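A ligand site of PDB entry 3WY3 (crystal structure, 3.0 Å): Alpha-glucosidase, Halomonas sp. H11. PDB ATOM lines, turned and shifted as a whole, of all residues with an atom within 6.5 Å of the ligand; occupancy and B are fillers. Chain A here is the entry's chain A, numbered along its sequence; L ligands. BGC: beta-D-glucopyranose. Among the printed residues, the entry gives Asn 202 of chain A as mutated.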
ATOM      1  N   TYR A  17     -13.613 -25.280  16.569  1.00  0.00           N
ATOM      2  CA  TYR A  17     -13.717 -24.682  15.234  1.00  0.00           C
ATOM      3  C   TYR A  17     -12.352 -24.101  14.882  1.00  0.00           C
ATOM      4  O   TYR A  17     -12.035 -22.975  15.292  1.00  0.00           O
ATOM      5  CB  TYR A  17     -14.805 -23.606  15.196  1.00  0.00           C
ATOM      6  CG  TYR A  17     -15.205 -23.166  13.813  1.00  0.00           C
ATOM      7  CD1 TYR A  17     -16.001 -23.964  13.001  1.00  0.00           C
ATOM      8  CD2 TYR A  17     -14.810 -21.923  13.314  1.00  0.00           C
ATOM      9  CE1 TYR A  17     -16.377 -23.560  11.738  1.00  0.00           C
ATOM     10  CE2 TYR A  17     -15.189 -21.509  12.051  1.00  0.00           C
ATOM     11  CZ  TYR A  17     -15.963 -22.326  11.269  1.00  0.00           C
ATOM     12  OH  TYR A  17     -16.341 -21.912  10.007  1.00  0.00           O
ATOM     13  N   TRP A  51     -13.909 -32.813  18.951  1.00  0.00           N
ATOM     14  CA  TRP A  51     -14.386 -32.945  17.583  1.00  0.00           C
ATOM     15  C   TRP A  51     -13.867 -31.756  16.795  1.00  0.00           C
ATOM     16  O   TRP A  51     -14.196 -30.605  17.094  1.00  0.00           O
ATOM     17  CB  TRP A  51     -15.923 -33.045  17.531  1.00  0.00           C
ATOM     18  CG  TRP A  51     -16.591 -32.482  16.288  1.00  0.00           C
ATOM     19  CD1 TRP A  51     -16.112 -32.493  15.008  1.00  0.00           C
ATOM     20  CD2 TRP A  51     -17.862 -31.826  16.232  1.00  0.00           C
ATOM     21  NE1 TRP A  51     -17.000 -31.880  14.165  1.00  0.00           N
ATOM     22  CE2 TRP A  51     -18.081 -31.466  14.888  1.00  0.00           C
ATOM     23  CE3 TRP A  51     -18.832 -31.518  17.186  1.00  0.00           C
ATOM     24  CZ2 TRP A  51     -19.237 -30.798  14.480  1.00  0.00           C
ATOM     25  CZ3 TRP A  51     -19.975 -30.858  16.778  1.00  0.00           C
ATOM     26  CH2 TRP A  51     -20.170 -30.512  15.435  1.00  0.00           C
ATOM     27  N   ASP A  62     -17.165 -22.480   1.943  1.00  0.00           N
ATOM     28  CA  ASP A  62     -18.013 -22.791   3.087  1.00  0.00           C
ATOM     29  C   ASP A  62     -17.092 -23.125   4.251  1.00  0.00           C
ATOM     30  O   ASP A  62     -17.443 -23.914   5.133  1.00  0.00           O
ATOM     31  CB  ASP A  62     -18.974 -23.930   2.774  1.00  0.00           C
ATOM     32  CG  ASP A  62     -20.046 -24.096   3.833  1.00  0.00           C
ATOM     33  OD1 ASP A  62     -20.229 -23.173   4.655  1.00  0.00           O
ATOM     34  OD2 ASP A  62     -20.703 -25.165   3.852  1.00  0.00           O
ATOM     35  N   TYR A  65     -16.013 -26.948   4.746  1.00  0.00           N
ATOM     36  CA  TYR A  65     -17.045 -27.928   4.425  1.00  0.00           C
ATOM     37  C   TYR A  65     -17.206 -28.130   2.928  1.00  0.00           C
ATOM     38  O   TYR A  65     -18.053 -28.915   2.487  1.00  0.00           O
ATOM     39  CB  TYR A  65     -18.371 -27.529   5.062  1.00  0.00           C
ATOM     40  CG  TYR A  65     -18.428 -27.808   6.540  1.00  0.00           C
ATOM     41  CD1 TYR A  65     -18.787 -29.061   7.022  1.00  0.00           C
ATOM     42  CD2 TYR A  65     -18.101 -26.823   7.471  1.00  0.00           C
ATOM     43  CE1 TYR A  65     -18.830 -29.334   8.371  1.00  0.00           C
ATOM     44  CE2 TYR A  65     -18.146 -27.088   8.831  1.00  0.00           C
ATOM     45  CZ  TYR A  65     -18.511 -28.338   9.272  1.00  0.00           C
ATOM     46  OH  TYR A  65     -18.556 -28.602  10.622  1.00  0.00           O
ATOM     47  N   ASP A  66     -16.401 -27.417   2.142  1.00  0.00           N
ATOM     48  CA  ASP A  66     -16.290 -27.710   0.721  1.00  0.00           C
ATOM     49  C   ASP A  66     -14.915 -28.329   0.458  1.00  0.00           C
ATOM     50  O   ASP A  66     -13.938 -27.621   0.204  1.00  0.00           O
ATOM     51  CB  ASP A  66     -16.502 -26.441  -0.119  1.00  0.00           C
ATOM     52  CG  ASP A  66     -15.638 -25.279   0.339  1.00  0.00           C
ATOM     53  OD1 ASP A  66     -15.517 -25.072   1.570  1.00  0.00           O
ATOM     54  OD2 ASP A  66     -15.079 -24.581  -0.534  1.00  0.00           O
ATOM     55  N   ASP A 100     -14.310 -34.124  11.477  1.00  0.00           N
ATOM     56  CA  ASP A 100     -15.439 -34.047  10.576  1.00  0.00           C
ATOM     57  C   ASP A 100     -15.248 -34.919   9.346  1.00  0.00           C
ATOM     58  O   ASP A 100     -14.117 -35.138   8.904  1.00  0.00           O
ATOM     59  CB  ASP A 100     -15.687 -32.596  10.139  1.00  0.00           C
ATOM     60  CG  ASP A 100     -17.032 -32.071  10.597  1.00  0.00           C
ATOM     61  OD1 ASP A 100     -18.047 -32.425   9.968  1.00  0.00           O
ATOM     62  OD2 ASP A 100     -17.065 -31.289  11.578  1.00  0.00           O
ATOM     63  N   VAL A 102     -17.123 -34.900   5.551  1.00  0.00           N
ATOM     64  CA  VAL A 102     -18.124 -34.313   4.663  1.00  0.00           C
ATOM     65  C   VAL A 102     -18.188 -35.133   3.384  1.00  0.00           C
ATOM     66  O   VAL A 102     -17.679 -34.723   2.340  1.00  0.00           O
ATOM     67  CB  VAL A 102     -17.788 -32.843   4.337  1.00  0.00           C
ATOM     68  CG1 VAL A 102     -18.991 -32.155   3.694  1.00  0.00           C
ATOM     69  CG2 VAL A 102     -17.366 -32.113   5.600  1.00  0.00           C
ATOM     70  N   HIS A 105     -21.094 -34.359   0.135  1.00  0.00           N
ATOM     71  CA  HIS A 105     -20.826 -33.485  -0.999  1.00  0.00           C
ATOM     72  C   HIS A 105     -19.377 -33.009  -0.991  1.00  0.00           C
ATOM     73  O   HIS A 105     -18.760 -32.904   0.064  1.00  0.00           O
ATOM     74  CB  HIS A 105     -21.777 -32.286  -0.968  1.00  0.00           C
ATOM     75  CG  HIS A 105     -21.821 -31.592   0.356  1.00  0.00           C
ATOM     76  ND1 HIS A 105     -22.805 -31.837   1.293  1.00  0.00           N
ATOM     77  CD2 HIS A 105     -21.005 -30.659   0.903  1.00  0.00           C
ATOM     78  CE1 HIS A 105     -22.592 -31.081   2.356  1.00  0.00           C
ATOM     79  NE2 HIS A 105     -21.511 -30.359   2.145  1.00  0.00           N
ATOM     80  N   PHE A 147     -28.711 -22.784   1.074  1.00  0.00           N
ATOM     81  CA  PHE A 147     -27.957 -21.539   1.005  1.00  0.00           C
ATOM     82  C   PHE A 147     -28.486 -20.609  -0.099  1.00  0.00           C
ATOM     83  O   PHE A 147     -27.803 -19.682  -0.517  1.00  0.00           O
ATOM     84  CB  PHE A 147     -26.473 -21.820   0.773  1.00  0.00           C
ATOM     85  CG  PHE A 147     -25.802 -22.481   1.943  1.00  0.00           C
ATOM     86  CD1 PHE A 147     -26.407 -22.529   3.184  1.00  0.00           C
ATOM     87  CD2 PHE A 147     -24.556 -23.061   1.794  1.00  0.00           C
ATOM     88  CE1 PHE A 147     -25.788 -23.142   4.254  1.00  0.00           C
ATOM     89  CE2 PHE A 147     -23.924 -23.680   2.864  1.00  0.00           C
ATOM     90  CZ  PHE A 147     -24.553 -23.715   4.104  1.00  0.00           C
ATOM     91  N   PHE A 166     -26.378 -27.439  -0.735  1.00  0.00           N
ATOM     92  CA  PHE A 166     -25.800 -26.201  -0.225  1.00  0.00           C
ATOM     93  C   PHE A 166     -25.274 -25.322  -1.353  1.00  0.00           C
ATOM     94  O   PHE A 166     -25.964 -25.119  -2.358  1.00  0.00           O
ATOM     95  CB  PHE A 166     -24.697 -26.514   0.787  1.00  0.00           C
ATOM     96  CG  PHE A 166     -25.173 -27.362   1.943  1.00  0.00           C
ATOM     97  CD1 PHE A 166     -25.795 -26.767   3.026  1.00  0.00           C
ATOM     98  CD2 PHE A 166     -25.002 -28.728   1.927  1.00  0.00           C
ATOM     99  CE1 PHE A 166     -26.234 -27.544   4.084  1.00  0.00           C
ATOM    100  CE2 PHE A 166     -25.441 -29.505   2.984  1.00  0.00           C
ATOM    101  CZ  PHE A 166     -26.054 -28.908   4.069  1.00  0.00           C
ATOM    102  N   LEU A 167     -24.067 -24.790  -1.190  1.00  0.00           N
ATOM    103  CA  LEU A 167     -23.466 -23.903  -2.188  1.00  0.00           C
ATOM    104  C   LEU A 167     -23.420 -24.527  -3.584  1.00  0.00           C
ATOM    105  O   LEU A 167     -23.437 -25.743  -3.733  1.00  0.00           O
ATOM    106  CB  LEU A 167     -22.048 -23.514  -1.779  1.00  0.00           C
ATOM    107  CG  LEU A 167     -21.864 -22.659  -0.524  1.00  0.00           C
ATOM    108  CD1 LEU A 167     -20.384 -22.384  -0.285  1.00  0.00           C
ATOM    109  CD2 LEU A 167     -22.635 -21.356  -0.646  1.00  0.00           C
ATOM    110  N   GLN A 170     -20.600 -26.683  -3.982  1.00  0.00           N
ATOM    111  CA  GLN A 170     -20.656 -27.923  -3.216  1.00  0.00           C
ATOM    112  C   GLN A 170     -21.619 -28.941  -3.828  1.00  0.00           C
ATOM    113  O   GLN A 170     -22.681 -29.210  -3.287  1.00  0.00           O
ATOM    114  CB  GLN A 170     -21.080 -27.642  -1.766  1.00  0.00           C
ATOM    115  CG  GLN A 170     -20.012 -26.939  -0.939  1.00  0.00           C
ATOM    116  CD  GLN A 170     -20.514 -26.516   0.429  1.00  0.00           C
ATOM    117  OE1 GLN A 170     -21.540 -25.842   0.541  1.00  0.00           O
ATOM    118  NE2 GLN A 170     -19.792 -26.900   1.466  1.00  0.00           N
ATOM    119  N   ARG A 200     -17.386 -37.081  13.156  1.00  0.00           N
ATOM    120  CA  ARG A 200     -18.682 -36.412  13.109  1.00  0.00           C
ATOM    121  C   ARG A 200     -19.161 -36.412  11.665  1.00  0.00           C
ATOM    122  O   ARG A 200     -18.504 -35.855  10.795  1.00  0.00           O
ATOM    123  CB  ARG A 200     -18.581 -34.994  13.664  1.00  0.00           C
ATOM    124  CG  ARG A 200     -19.890 -34.193  13.622  1.00  0.00           C
ATOM    125  CD  ARG A 200     -19.985 -33.342  12.369  1.00  0.00           C
ATOM    126  NE  ARG A 200     -21.088 -32.383  12.437  1.00  0.00           N
ATOM    127  CZ  ARG A 200     -21.349 -31.491  11.497  1.00  0.00           C
ATOM    128  NH1 ARG A 200     -20.590 -31.426  10.405  1.00  0.00           N
ATOM    129  NH2 ARG A 200     -22.359 -30.650  11.640  1.00  0.00           N
ATOM    130  N   ASN A 202     -21.112 -35.145   8.833  1.00  0.00           N
ATOM    131  CA  ASN A 202     -21.851 -34.002   8.301  1.00  0.00           C
ATOM    132  C   ASN A 202     -23.092 -34.413   7.522  1.00  0.00           C
ATOM    133  O   ASN A 202     -22.988 -35.211   6.586  1.00  0.00           O
ATOM    134  CB  ASN A 202     -20.936 -33.176   7.397  1.00  0.00           C
ATOM    135  CG  ASN A 202     -21.496 -31.801   7.113  1.00  0.00           C
ATOM    136  OD1 ASN A 202     -22.071 -31.164   7.994  1.00  0.00           O
ATOM    137  ND2 ASN A 202     -21.348 -31.344   5.877  1.00  0.00           N
ATOM    138  N   THR A 203     -24.232 -33.835   7.894  1.00  0.00           N
ATOM    139  CA  THR A 203     -25.524 -34.105   7.239  1.00  0.00           C
ATOM    140  C   THR A 203     -25.706 -35.583   6.871  1.00  0.00           C
ATOM    141  O   THR A 203     -25.888 -35.916   5.709  1.00  0.00           O
ATOM    142  CB  THR A 203     -25.700 -33.253   5.968  1.00  0.00           C
ATOM    143  OG1 THR A 203     -24.572 -33.413   5.108  1.00  0.00           O
ATOM    144  CG2 THR A 203     -25.856 -31.791   6.331  1.00  0.00           C
ATOM    145  N   GLU A 271     -24.891 -35.891  12.197  1.00  0.00           N
ATOM    146  CA  GLU A 271     -25.682 -34.671  12.235  1.00  0.00           C
ATOM    147  C   GLU A 271     -26.990 -34.861  11.466  1.00  0.00           C
ATOM    148  O   GLU A 271     -26.986 -35.174  10.275  1.00  0.00           O
ATOM    149  CB  GLU A 271     -24.903 -33.506  11.653  1.00  0.00           C
ATOM    150  CG  GLU A 271     -25.701 -32.221  11.537  1.00  0.00           C
ATOM    151  CD  GLU A 271     -25.149 -31.309  10.467  1.00  0.00           C
ATOM    152  OE1 GLU A 271     -24.213 -31.732   9.759  1.00  0.00           O
ATOM    153  OE2 GLU A 271     -25.657 -30.174  10.331  1.00  0.00           O
ATOM    154  N   TYR A 295     -26.875 -36.258  16.784  1.00  0.00           N
ATOM    155  CA  TYR A 295     -27.470 -35.094  17.423  1.00  0.00           C
ATOM    156  C   TYR A 295     -28.473 -34.401  16.507  1.00  0.00           C
ATOM    157  O   TYR A 295     -28.387 -34.491  15.290  1.00  0.00           O
ATOM    158  CB  TYR A 295     -26.385 -34.114  17.891  1.00  0.00           C
ATOM    159  CG  TYR A 295     -25.732 -33.268  16.812  1.00  0.00           C
ATOM    160  CD1 TYR A 295     -26.283 -32.049  16.439  1.00  0.00           C
ATOM    161  CD2 TYR A 295     -24.561 -33.678  16.190  1.00  0.00           C
ATOM    162  CE1 TYR A 295     -25.701 -31.263  15.468  1.00  0.00           C
ATOM    163  CE2 TYR A 295     -23.966 -32.898  15.209  1.00  0.00           C
ATOM    164  CZ  TYR A 295     -24.538 -31.686  14.853  1.00  0.00           C
ATOM    165  OH  TYR A 295     -23.954 -30.910  13.881  1.00  0.00           O
ATOM    166  N   PHE A 297     -31.355 -30.749  16.067  1.00  0.00           N
ATOM    167  CA  PHE A 297     -31.477 -29.318  16.308  1.00  0.00           C
ATOM    168  C   PHE A 297     -32.600 -28.992  17.289  1.00  0.00           C
ATOM    169  O   PHE A 297     -32.994 -27.831  17.421  1.00  0.00           O
ATOM    170  CB  PHE A 297     -31.685 -28.564  14.992  1.00  0.00           C
ATOM    171  CG  PHE A 297     -30.409 -28.231  14.277  1.00  0.00           C
ATOM    172  CD1 PHE A 297     -29.968 -26.920  14.175  1.00  0.00           C
ATOM    173  CD2 PHE A 297     -29.636 -29.229  13.707  1.00  0.00           C
ATOM    174  CE1 PHE A 297     -28.798 -26.612  13.528  1.00  0.00           C
ATOM    175  CE2 PHE A 297     -28.463 -28.929  13.049  1.00  0.00           C
ATOM    176  CZ  PHE A 297     -28.033 -27.624  12.965  1.00  0.00           C
ATOM    177  N   ASN A 331     -23.257 -24.896  18.470  1.00  0.00           N
ATOM    178  CA  ASN A 331     -22.225 -25.291  17.522  1.00  0.00           C
ATOM    179  C   ASN A 331     -21.910 -24.151  16.557  1.00  0.00           C
ATOM    180  O   ASN A 331     -22.295 -22.998  16.799  1.00  0.00           O
ATOM    181  CB  ASN A 331     -22.627 -26.562  16.762  1.00  0.00           C
ATOM    182  CG  ASN A 331     -23.964 -26.410  16.031  1.00  0.00           C
ATOM    183  OD1 ASN A 331     -24.409 -25.315  15.725  1.00  0.00           O
ATOM    184  ND2 ASN A 331     -24.596 -27.547  15.741  1.00  0.00           N
ATOM    185  N   HIS A 332     -21.206 -24.454  15.476  1.00  0.00           N
ATOM    186  CA  HIS A 332     -20.775 -23.449  14.516  1.00  0.00           C
ATOM    187  C   HIS A 332     -21.889 -23.001  13.570  1.00  0.00           C
ATOM    188  O   HIS A 332     -21.662 -22.172  12.690  1.00  0.00           O
ATOM    189  CB  HIS A 332     -19.592 -23.974  13.709  1.00  0.00           C
ATOM    190  CG  HIS A 332     -19.923 -25.156  12.866  1.00  0.00           C
ATOM    191  ND1 HIS A 332     -20.265 -26.377  13.394  1.00  0.00           N
ATOM    192  CD2 HIS A 332     -19.960 -25.307  11.508  1.00  0.00           C
ATOM    193  CE1 HIS A 332     -20.503 -27.241  12.416  1.00  0.00           C
ATOM    194  NE2 HIS A 332     -20.328 -26.607  11.265  1.00  0.00           N
ATOM    195  N   ASP A 333     -23.091 -23.553  13.739  1.00  0.00           N
ATOM    196  CA  ASP A 333     -24.194 -23.250  12.828  1.00  0.00           C
ATOM    197  C   ASP A 333     -25.327 -22.468  13.478  1.00  0.00           C
ATOM    198  O   ASP A 333     -26.245 -22.023  12.794  1.00  0.00           O
ATOM    199  CB  ASP A 333     -24.750 -24.536  12.243  1.00  0.00           C
ATOM    200  CG  ASP A 333     -23.782 -25.208  11.296  1.00  0.00           C
ATOM    201  OD1 ASP A 333     -23.057 -24.501  10.572  1.00  0.00           O
ATOM    202  OD2 ASP A 333     -23.748 -26.457  11.301  1.00  0.00           O
ATOM    203  N   ASP A 387     -19.274 -15.664   6.241  1.00  0.00           N
ATOM    204  CA  ASP A 387     -20.181 -16.754   5.899  1.00  0.00           C
ATOM    205  C   ASP A 387     -21.116 -16.374   4.750  1.00  0.00           C
ATOM    206  O   ASP A 387     -21.891 -15.428   4.878  1.00  0.00           O
ATOM    207  CB  ASP A 387     -20.994 -17.170   7.135  1.00  0.00           C
ATOM    208  CG  ASP A 387     -21.923 -18.336   6.873  1.00  0.00           C
ATOM    209  OD1 ASP A 387     -21.681 -19.095   5.914  1.00  0.00           O
ATOM    210  OD2 ASP A 387     -22.894 -18.498   7.628  1.00  0.00           O
ATOM    211  N   ARG A 400     -23.877 -17.194  10.198  1.00  0.00           N
ATOM    212  CA  ARG A 400     -23.395 -17.953  11.338  1.00  0.00           C
ATOM    213  C   ARG A 400     -22.106 -17.386  11.918  1.00  0.00           C
ATOM    214  O   ARG A 400     -21.517 -17.960  12.828  1.00  0.00           O
ATOM    215  CB  ARG A 400     -23.191 -19.418  10.929  1.00  0.00           C
ATOM    216  CG  ARG A 400     -24.463 -20.130  10.495  1.00  0.00           C
ATOM    217  CD  ARG A 400     -24.157 -21.399   9.725  1.00  0.00           C
ATOM    218  NE  ARG A 400     -23.407 -21.146   8.493  1.00  0.00           N
ATOM    219  CZ  ARG A 400     -22.988 -22.100   7.670  1.00  0.00           C
ATOM    220  NH1 ARG A 400     -23.240 -23.376   7.937  1.00  0.00           N
ATOM    221  NH2 ARG A 400     -22.305 -21.774   6.573  1.00  0.00           N
ATOM    222  N   ARG A 404     -18.817 -17.796  15.350  1.00  0.00           N
ATOM    223  CA  ARG A 404     -17.547 -18.257  14.782  1.00  0.00           C
ATOM    224  C   ARG A 404     -16.429 -17.259  15.042  1.00  0.00           C
ATOM    225  O   ARG A 404     -15.327 -17.394  14.497  1.00  0.00           O
ATOM    226  CB  ARG A 404     -17.695 -18.508  13.279  1.00  0.00           C
ATOM    227  CG  ARG A 404     -18.379 -19.820  12.933  1.00  0.00           C
ATOM    228  CD  ARG A 404     -19.166 -19.708  11.634  1.00  0.00           C
ATOM    229  NE  ARG A 404     -18.652 -20.595  10.596  1.00  0.00           N
ATOM    230  CZ  ARG A 404     -19.413 -21.402   9.857  1.00  0.00           C
ATOM    231  NH1 ARG A 404     -20.717 -21.431  10.029  1.00  0.00           N
ATOM    232  NH2 ARG A 404     -18.852 -22.163   8.930  1.00  0.00           N
HETATM  233  C2  BGC L   1     -22.610 -28.105   8.522  1.00  0.00           C
HETATM  234  C3  BGC L   1     -22.279 -26.674   8.150  1.00  0.00           C
HETATM  235  C4  BGC L   1     -22.087 -26.584   6.642  1.00  0.00           C
HETATM  236  C5  BGC L   1     -23.184 -27.309   5.849  1.00  0.00           C
HETATM  237  C6  BGC L   1     -22.733 -27.542   4.418  1.00  0.00           C
HETATM  238  C1  BGC L   1     -23.869 -28.503   7.773  1.00  0.00           C
HETATM  239  O1  BGC L   1     -24.305 -29.762   8.226  1.00  0.00           O
HETATM  240  O2  BGC L   1     -22.775 -28.280   9.902  1.00  0.00           O
HETATM  241  O3  BGC L   1     -21.107 -26.260   8.811  1.00  0.00           O
HETATM  242  O4  BGC L   1     -22.055 -25.229   6.241  1.00  0.00           O
HETATM  243  O5  BGC L   1     -23.531 -28.564   6.403  1.00  0.00           O
HETATM  244  O6  BGC L   1     -21.445 -28.103   4.396  1.00  0.00           O
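NH2 of Arg 400 is in salt-bridge range of OD1 of Asp 387, at 2.8 Å. NH1 of Arg 400 lies within salt-bridge range of OD1 of Asp 333, 2.9 Å away. The backbone carbonyl oxygen of His 332 sits at hydrogen-bond distance from the guanidinium group of Arg 404 (2.9 Å). OD1 of Asn 202 sits at hydrogen-bond distance from NH1 of Arg 200 (2.8 Å). OE1 of Glu 271 lies within hydrogen-bond range of N of Thr 203. The side-chain carboxylate (OD2) of Asp 333 lies within hydrogen-bond range of a ring nitrogen (NE2) of His 332. OE1 of Gln 170 lies within hydrogen-bond range of N of Leu 167, 3.2 Å away. The guanidinium group (NH1) of Arg 200 is in salt-bridge range of the side-chain carboxylate (OD1) of Asp 100 (2.8 Å).
Residues that only touch the ligand: Tyr 65 (3.1 Å), Phe 147 (3.6 Å), Phe 166 (3.5 Å), Gln 170 (3.6 Å) and Thr 203 (3.2 Å). 13 residues have an atom within 4 Å of the ligand: Asp 62, Tyr 65, His 105, Phe 147, Phe 166, Gln 170, Arg 200, Asn 202, Thr 203, Glu 271, His 332, Asp 333 and Arg 400.
The side-chain carboxylate (OE1) of Glu 271 sits at hydrogen-bond distance from an oxygen (O1) of the ligand (2.5 Å). The guanidinium group (NH2) of Arg 200 sits at hydrogen-bond distance from an oxygen (O2) of the ligand. O4 of the ligand is in hydrogen-bond range of OD2 of Asp 62, at 2.7 Å. The side-chain amide oxygen of Asn 202 sits at hydrogen-bond distance from an oxygen (O1) of the ligand. A ring nitrogen (NE2) of His 332 lies within hydrogen-bond range of an oxygen (O3) of the ligand (2.6 Å). O6 of the ligand lies within hydrogen-bond range of NE2 of His 105 (3.2 Å). The side-chain carboxylate (OD2) of Asp 333 is in hydrogen-bond range of an oxygen (O2) of the ligand (2.5 Å). An oxygen (O4) of the ligand is in hydrogen-bond range of the guanidinium group (NH1) of Arg 400 (2.8 Å).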
